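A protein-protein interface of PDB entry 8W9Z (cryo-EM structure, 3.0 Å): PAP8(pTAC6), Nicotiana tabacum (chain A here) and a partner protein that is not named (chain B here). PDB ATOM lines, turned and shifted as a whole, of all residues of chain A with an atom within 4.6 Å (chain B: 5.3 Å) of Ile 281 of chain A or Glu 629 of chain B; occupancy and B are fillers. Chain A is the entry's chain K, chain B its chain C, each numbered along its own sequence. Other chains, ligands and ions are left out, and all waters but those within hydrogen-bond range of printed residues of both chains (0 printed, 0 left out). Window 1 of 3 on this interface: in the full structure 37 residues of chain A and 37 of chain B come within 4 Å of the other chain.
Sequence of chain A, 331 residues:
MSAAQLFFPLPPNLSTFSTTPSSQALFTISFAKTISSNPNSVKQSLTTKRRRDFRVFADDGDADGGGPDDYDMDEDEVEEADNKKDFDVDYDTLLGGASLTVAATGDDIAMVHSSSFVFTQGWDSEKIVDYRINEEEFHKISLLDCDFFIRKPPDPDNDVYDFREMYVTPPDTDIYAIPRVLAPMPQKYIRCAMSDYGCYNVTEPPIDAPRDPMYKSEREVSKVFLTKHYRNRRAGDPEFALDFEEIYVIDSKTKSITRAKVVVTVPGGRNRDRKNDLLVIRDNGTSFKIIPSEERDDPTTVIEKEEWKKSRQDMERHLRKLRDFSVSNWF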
ATOM      1  N   PHE A 225     -16.500  33.538 -31.399  1.00  0.00           N
ATOM      2  CA  PHE A 225     -16.189  33.980 -30.047  1.00  0.00           C
ATOM      3  C   PHE A 225     -14.741  33.641 -29.719  1.00  0.00           C
ATOM      4  O   PHE A 225     -14.288  32.520 -29.974  1.00  0.00           O
ATOM      5  CB  PHE A 225     -17.125  33.324 -29.034  1.00  0.00           C
ATOM      6  CG  PHE A 225     -18.580  33.553 -29.316  1.00  0.00           C
ATOM      7  CD1 PHE A 225     -19.032  34.792 -29.732  1.00  0.00           C
ATOM      8  CD2 PHE A 225     -19.496  32.526 -29.175  1.00  0.00           C
ATOM      9  CE1 PHE A 225     -20.370  35.003 -29.994  1.00  0.00           C
ATOM     10  CE2 PHE A 225     -20.833  32.732 -29.438  1.00  0.00           C
ATOM     11  CZ  PHE A 225     -21.271  33.972 -29.849  1.00  0.00           C
ATOM     12  N   LEU A 279     -21.112  29.921 -19.018  1.00  0.00           N
ATOM     13  CA  LEU A 279     -21.567  31.043 -19.832  1.00  0.00           C
ATOM     14  C   LEU A 279     -22.774  30.604 -20.652  1.00  0.00           C
ATOM     15  O   LEU A 279     -22.675  29.687 -21.473  1.00  0.00           O
ATOM     16  CB  LEU A 279     -20.446  31.537 -20.739  1.00  0.00           C
ATOM     17  CG  LEU A 279     -20.849  32.621 -21.739  1.00  0.00           C
ATOM     18  CD1 LEU A 279     -20.984  33.969 -21.050  1.00  0.00           C
ATOM     19  CD2 LEU A 279     -19.861  32.689 -22.886  1.00  0.00           C
ATOM     20  N   VAL A 280     -23.912  31.252 -20.431  1.00  0.00           N
ATOM     21  CA  VAL A 280     -25.134  30.979 -21.177  1.00  0.00           C
ATOM     22  C   VAL A 280     -25.314  32.082 -22.209  1.00  0.00           C
ATOM     23  O   VAL A 280     -25.369  33.267 -21.861  1.00  0.00           O
ATOM     24  CB  VAL A 280     -26.352  30.887 -20.246  1.00  0.00           C
ATOM     25  CG1 VAL A 280     -27.616  30.642 -21.053  1.00  0.00           C
ATOM     26  CG2 VAL A 280     -26.148  29.787 -19.221  1.00  0.00           C
ATOM     27  N   ILE A 281     -25.406  31.695 -23.480  1.00  0.00           N
ATOM     28  CA  ILE A 281     -25.539  32.629 -24.591  1.00  0.00           C
ATOM     29  C   ILE A 281     -26.937  32.488 -25.174  1.00  0.00           C
ATOM     30  O   ILE A 281     -27.361  31.379 -25.521  1.00  0.00           O
ATOM     31  CB  ILE A 281     -24.468  32.381 -25.666  1.00  0.00           C
ATOM     32  CG1 ILE A 281     -23.072  32.411 -25.045  1.00  0.00           C
ATOM     33  CG2 ILE A 281     -24.578  33.411 -26.774  1.00  0.00           C
ATOM     34  CD1 ILE A 281     -21.963  32.130 -26.032  1.00  0.00           C
ATOM     35  N   ARG A 282     -27.650  33.608 -25.283  1.00  0.00           N
ATOM     36  CA  ARG A 282     -29.004  33.622 -25.819  1.00  0.00           C
ATOM     37  C   ARG A 282     -29.179  34.855 -26.696  1.00  0.00           C
ATOM     38  O   ARG A 282     -28.277  35.687 -26.823  1.00  0.00           O
ATOM     39  CB  ARG A 282     -30.051  33.600 -24.699  1.00  0.00           C
ATOM     40  CG  ARG A 282     -30.038  32.346 -23.844  1.00  0.00           C
ATOM     41  CD  ARG A 282     -31.174  32.342 -22.832  1.00  0.00           C
ATOM     42  NE  ARG A 282     -32.486  32.282 -23.471  1.00  0.00           N
ATOM     43  CZ  ARG A 282     -33.284  33.330 -23.646  1.00  0.00           C
ATOM     44  NH1 ARG A 282     -32.908  34.530 -23.225  1.00  0.00           N
ATOM     45  NH2 ARG A 282     -34.460  33.180 -24.239  1.00  0.00           N
ATOM     46  N   GLY A 285     -26.720  35.331 -29.872  1.00  0.00           N
ATOM     47  CA  GLY A 285     -25.359  35.694 -29.523  1.00  0.00           C
ATOM     48  C   GLY A 285     -25.188  37.109 -29.021  1.00  0.00           C
ATOM     49  O   GLY A 285     -24.134  37.712 -29.240  1.00  0.00           O
ATOM     50  N   SER A 287     -26.692  38.029 -25.646  1.00  0.00           N
ATOM     51  CA  SER A 287     -26.859  38.012 -24.200  1.00  0.00           C
ATOM     52  C   SER A 287     -25.881  37.018 -23.593  1.00  0.00           C
ATOM     53  O   SER A 287     -25.838  35.855 -24.004  1.00  0.00           O
ATOM     54  CB  SER A 287     -28.295  37.646 -23.816  1.00  0.00           C
ATOM     55  OG  SER A 287     -29.218  38.576 -24.356  1.00  0.00           O
ATOM     56  N   PHE A 288     -25.100  37.477 -22.619  1.00  0.00           N
ATOM     57  CA  PHE A 288     -24.113  36.647 -21.941  1.00  0.00           C
ATOM     58  C   PHE A 288     -24.355  36.705 -20.441  1.00  0.00           C
ATOM     59  O   PHE A 288     -24.497  37.792 -19.874  1.00  0.00           O
ATOM     60  CB  PHE A 288     -22.687  37.105 -22.263  1.00  0.00           C
ATOM     61  CG  PHE A 288     -22.312  36.960 -23.709  1.00  0.00           C
ATOM     62  CD1 PHE A 288     -22.626  37.951 -24.624  1.00  0.00           C
ATOM     63  CD2 PHE A 288     -21.638  35.836 -24.154  1.00  0.00           C
ATOM     64  CE1 PHE A 288     -22.280  37.821 -25.952  1.00  0.00           C
ATOM     65  CE2 PHE A 288     -21.289  35.701 -25.480  1.00  0.00           C
ATOM     66  CZ  PHE A 288     -21.611  36.694 -26.380  1.00  0.00           C
ATOM     67  N   VAL A 302     -35.118  23.936 -21.497  1.00  0.00           N
ATOM     68  CA  VAL A 302     -35.161  25.196 -22.234  1.00  0.00           C
ATOM     69  C   VAL A 302     -35.925  25.040 -23.544  1.00  0.00           C
ATOM     70  O   VAL A 302     -36.624  25.969 -23.978  1.00  0.00           O
ATOM     71  CB  VAL A 302     -33.736  25.737 -22.464  1.00  0.00           C
ATOM     72  CG1 VAL A 302     -33.136  26.204 -21.149  1.00  0.00           C
ATOM     73  CG2 VAL A 302     -32.854  24.681 -23.102  1.00  0.00           C
ATOM     74  N   PRO B 627     -28.793  28.379 -32.375  1.00  0.00           N
ATOM     75  CA  PRO B 627     -29.196  27.615 -31.190  1.00  0.00           C
ATOM     76  C   PRO B 627     -29.836  28.504 -30.135  1.00  0.00           C
ATOM     77  O   PRO B 627     -29.568  29.705 -30.055  1.00  0.00           O
ATOM     78  CB  PRO B 627     -27.878  27.012 -30.690  1.00  0.00           C
ATOM     79  CG  PRO B 627     -26.820  27.890 -31.258  1.00  0.00           C
ATOM     80  CD  PRO B 627     -27.338  28.318 -32.594  1.00  0.00           C
ATOM     81  N   ILE B 628     -30.696  27.893 -29.318  1.00  0.00           N
ATOM     82  CA  ILE B 628     -31.395  28.650 -28.286  1.00  0.00           C
ATOM     83  C   ILE B 628     -30.449  29.006 -27.144  1.00  0.00           C
ATOM     84  O   ILE B 628     -30.508  30.113 -26.597  1.00  0.00           O
ATOM     85  CB  ILE B 628     -32.629  27.872 -27.794  1.00  0.00           C
ATOM     86  CG1 ILE B 628     -32.232  26.508 -27.226  1.00  0.00           C
ATOM     87  CG2 ILE B 628     -33.620  27.680 -28.927  1.00  0.00           C
ATOM     88  CD1 ILE B 628     -33.402  25.693 -26.724  1.00  0.00           C
ATOM     89  N   GLU B 629     -29.556  28.088 -26.776  1.00  0.00           N
ATOM     90  CA  GLU B 629     -28.599  28.324 -25.706  1.00  0.00           C
ATOM     91  C   GLU B 629     -27.301  27.595 -26.024  1.00  0.00           C
ATOM     92  O   GLU B 629     -27.306  26.532 -26.648  1.00  0.00           O
ATOM     93  CB  GLU B 629     -29.127  27.860 -24.342  1.00  0.00           C
ATOM     94  CG  GLU B 629     -30.257  28.701 -23.772  1.00  0.00           C
ATOM     95  CD  GLU B 629     -30.546  28.376 -22.321  1.00  0.00           C
ATOM     96  OE1 GLU B 629     -31.160  29.218 -21.633  1.00  0.00           O
ATOM     97  OE2 GLU B 629     -30.154  27.281 -21.867  1.00  0.00           O
ATOM     98  N   VAL B 630     -26.190  28.180 -25.583  1.00  0.00           N
ATOM     99  CA  VAL B 630     -24.865  27.584 -25.714  1.00  0.00           C
ATOM    100  C   VAL B 630     -24.218  27.621 -24.338  1.00  0.00           C
ATOM    101  O   VAL B 630     -23.792  28.687 -23.877  1.00  0.00           O
ATOM    102  CB  VAL B 630     -23.994  28.312 -26.746  1.00  0.00           C
ATOM    103  CG1 VAL B 630     -22.613  27.682 -26.808  1.00  0.00           C
ATOM    104  CG2 VAL B 630     -24.655  28.289 -28.115  1.00  0.00           C
ATOM    105  N   HIS B 631     -24.146  26.465 -23.678  1.00  0.00           N
ATOM    106  CA  HIS B 631     -23.573  26.366 -22.336  1.00  0.00           C
ATOM    107  C   HIS B 631     -22.068  26.170 -22.469  1.00  0.00           C
ATOM    108  O   HIS B 631     -21.573  25.050 -22.598  1.00  0.00           O
ATOM    109  CB  HIS B 631     -24.221  25.231 -21.554  1.00  0.00           C
ATOM    110  CG  HIS B 631     -25.663  25.465 -21.233  1.00  0.00           C
ATOM    111  ND1 HIS B 631     -26.447  24.521 -20.606  1.00  0.00           N
ATOM    112  CD2 HIS B 631     -26.463  26.535 -21.449  1.00  0.00           C
ATOM    113  CE1 HIS B 631     -27.669  25.000 -20.451  1.00  0.00           C
ATOM    114  NE2 HIS B 631     -27.705  26.220 -20.954  1.00  0.00           N
ATOM    115  N   TYR B 632     -21.333  27.278 -22.425  1.00  0.00           N
ATOM    116  CA  TYR B 632     -19.881  27.268 -22.592  1.00  0.00           C
ATOM    117  C   TYR B 632     -19.246  27.168 -21.211  1.00  0.00           C
ATOM    118  O   TYR B 632     -19.195  28.151 -20.466  1.00  0.00           O
ATOM    119  CB  TYR B 632     -19.427  28.516 -23.340  1.00  0.00           C
ATOM    120  CG  TYR B 632     -18.001  28.467 -23.836  1.00  0.00           C
ATOM    121  CD1 TYR B 632     -16.951  28.882 -23.030  1.00  0.00           C
ATOM    122  CD2 TYR B 632     -17.706  28.015 -25.113  1.00  0.00           C
ATOM    123  CE1 TYR B 632     -15.647  28.842 -23.481  1.00  0.00           C
ATOM    124  CE2 TYR B 632     -16.404  27.971 -25.572  1.00  0.00           C
ATOM    125  CZ  TYR B 632     -15.378  28.385 -24.752  1.00  0.00           C
ATOM    126  OH  TYR B 632     -14.080  28.344 -25.205  1.00  0.00           O
ATOM    127  N   TYR B 639     -21.985  22.955 -24.945  1.00  0.00           N
ATOM    128  CA  TYR B 639     -23.143  22.256 -25.486  1.00  0.00           C
ATOM    129  C   TYR B 639     -23.995  23.244 -26.271  1.00  0.00           C
ATOM    130  O   TYR B 639     -24.472  24.238 -25.712  1.00  0.00           O
ATOM    131  CB  TYR B 639     -23.968  21.619 -24.369  1.00  0.00           C
ATOM    132  CG  TYR B 639     -23.169  20.792 -23.387  1.00  0.00           C
ATOM    133  CD1 TYR B 639     -22.577  21.377 -22.276  1.00  0.00           C
ATOM    134  CD2 TYR B 639     -23.020  19.425 -23.564  1.00  0.00           C
ATOM    135  CE1 TYR B 639     -21.850  20.625 -21.375  1.00  0.00           C
ATOM    136  CE2 TYR B 639     -22.296  18.663 -22.667  1.00  0.00           C
ATOM    137  CZ  TYR B 639     -21.714  19.268 -21.575  1.00  0.00           C
ATOM    138  OH  TYR B 639     -20.991  18.513 -20.680  1.00  0.00           O
ATOM    139  N   GLU B 640     -24.186  22.974 -27.559  1.00  0.00           N
ATOM    140  CA  GLU B 640     -25.032  23.794 -28.418  1.00  0.00           C
ATOM    141  C   GLU B 640     -26.419  23.163 -28.467  1.00  0.00           C
ATOM    142  O   GLU B 640     -26.613  22.125 -29.109  1.00  0.00           O
ATOM    143  CB  GLU B 640     -24.434  23.923 -29.816  1.00  0.00           C
ATOM    144  CG  GLU B 640     -23.106  24.658 -29.859  1.00  0.00           C
ATOM    145  CD  GLU B 640     -22.572  24.811 -31.269  1.00  0.00           C
ATOM    146  OE1 GLU B 640     -23.222  24.308 -32.210  1.00  0.00           O
ATOM    147  OE2 GLU B 640     -21.504  25.436 -31.438  1.00  0.00           O
ATOM    148  N   ILE B 641     -27.377  23.789 -27.794  1.00  0.00           N
ATOM    149  CA  ILE B 641     -28.736  23.270 -27.703  1.00  0.00           C
ATOM    150  C   ILE B 641     -29.579  23.920 -28.790  1.00  0.00           C
ATOM    151  O   ILE B 641     -29.765  25.141 -28.798  1.00  0.00           O
ATOM    152  CB  ILE B 641     -29.336  23.528 -26.315  1.00  0.00           C
ATOM    153  CG1 ILE B 641     -28.458  22.902 -25.231  1.00  0.00           C
ATOM    154  CG2 ILE B 641     -30.750  22.984 -26.242  1.00  0.00           C
ATOM    155  CD1 ILE B 641     -28.894  23.239 -23.825  1.00  0.00           C
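Of the 9 printed residues of chain B, 5 touch a printed residue of chain A.
Printed residues of chain B that touch a printed residue of chain A: Ile 628, Glu 629, Val 630, His 631 and Tyr 632.
Hydrophobic or aromatic side chains of chain B within 4 Å of the printed part of chain A: Ile 628, His 631 and Tyr 632.
Of the 9 printed residues of chain A, 5 touch a printed residue of chain B.
Printed residues of chain A that touch a printed residue of chain B: Leu 279, Val 280, Ile 281, Arg 282 and Val 302.
Hydrophobic or aromatic side chains of chain A within 4 Å of the printed part of chain B: Leu 279, Val 280, Ile 281 and Val 302.
Among the printed residues, 13 pairs touch across the chains.
Among the printed residues, Asp or Glu carboxylates within 4 Å of a Lys or Arg side-chain nitrogen of the other chain: Arg 282 of chain A with Glu 629 of chain B (3.8 Å).
Printed residues of chain B within 4 Å of Val 280 of chain A: Glu 629 (3.9 Å), Val 630 (3.8 Å) and His 631 (3.95 Å).
Of chain B, only Ile 628, Glu 629 and Val 630 come within 4 Å of Ile 281 of chain A.
Of the printed residues of chain B, Arg 282 of chain A touches Ile 628 (3.6 Å) and Glu 629 (3.3 Å).
Ser 287 of chain A touches none of the printed residues of chain B.
Phe 288 of chain A touches none of the printed residues of chain B.
Printed residues of chain B within 4 Å of Val 302 of chain A: Ile 628 and Glu 629.
Of the printed residues of chain A, Ile 628 of chain B touches Ile 281, Arg 282 and Val 302.
Of chain A, only Val 280 (3.9 Å), Ile 281 (3.3 Å), Arg 282 (3.3 Å) and Val 302 (3.3 Å) come within 4 Å of Glu 629 of chain B.
Of the printed residues of chain A, His 631 of chain B touches Leu 279 and Val 280.
The nearest printed residue of chain A that does not touch Glu 629 of chain B is Leu 279 of chain A (6.8 Å).
The nearest printed residue of chain A that does not touch Val 630 of chain B is Arg 282 of chain A (5.6 Å).
N of Ser 287 of chain A sits at hydrogen-bond distance from O of Arg 282 of chain A (3.1 Å).
O of Ile 641 of chain B is in hydrogen-bond range of N of Ile 628 of chain B (3.0 Å).
OE2 of Glu 629 of chain B lies within hydrogen-bond range of NE2 of His 631 of chain B, 2.8 Å away.
N of His 631 of chain B lies within hydrogen-bond range of O of Tyr 639 of chain B (3.0 Å).
The backbone carbonyl oxygen of Glu 629 of chain B is in hydrogen-bond range of the backbone NH of Ile 641 of chain B (3.0 Å).
The backbone NH (N) of Tyr 632 of chain B sits at hydrogen-bond distance from the backbone carbonyl oxygen (O) of Leu 279 of chain A (2.9 Å).
O of Val 630 of chain B sits close to O of Leu 279 of chain A.
The backbone NH (N) of Val 630 of chain B sits at hydrogen-bond distance from the backbone carbonyl oxygen (O) of Ile 281 of chain A.
The side-chain carboxylate of Glu 629 of chain B lies within salt-bridge range of the guanidinium group of Arg 282 of chain A (3.8 Å).
Among the printed residues, merely in contact across the chains: Val 302 of chain A with Glu 629 of chain B, Ile 281 of chain A with Glu 629 of chain B, Leu 279 of chain A with His 631 of chain B, Ile 281 of chain A with Ile 628 of chain B, Arg 282 of chain A with Ile 628 of chain B, Val 280 of chain A with Val 630 of chain B, Val 302 of chain A with Ile 628 of chain B, Val 280 of chain A with Glu 629 of chain B and Val 280 of chain A with His 631 of chain B.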
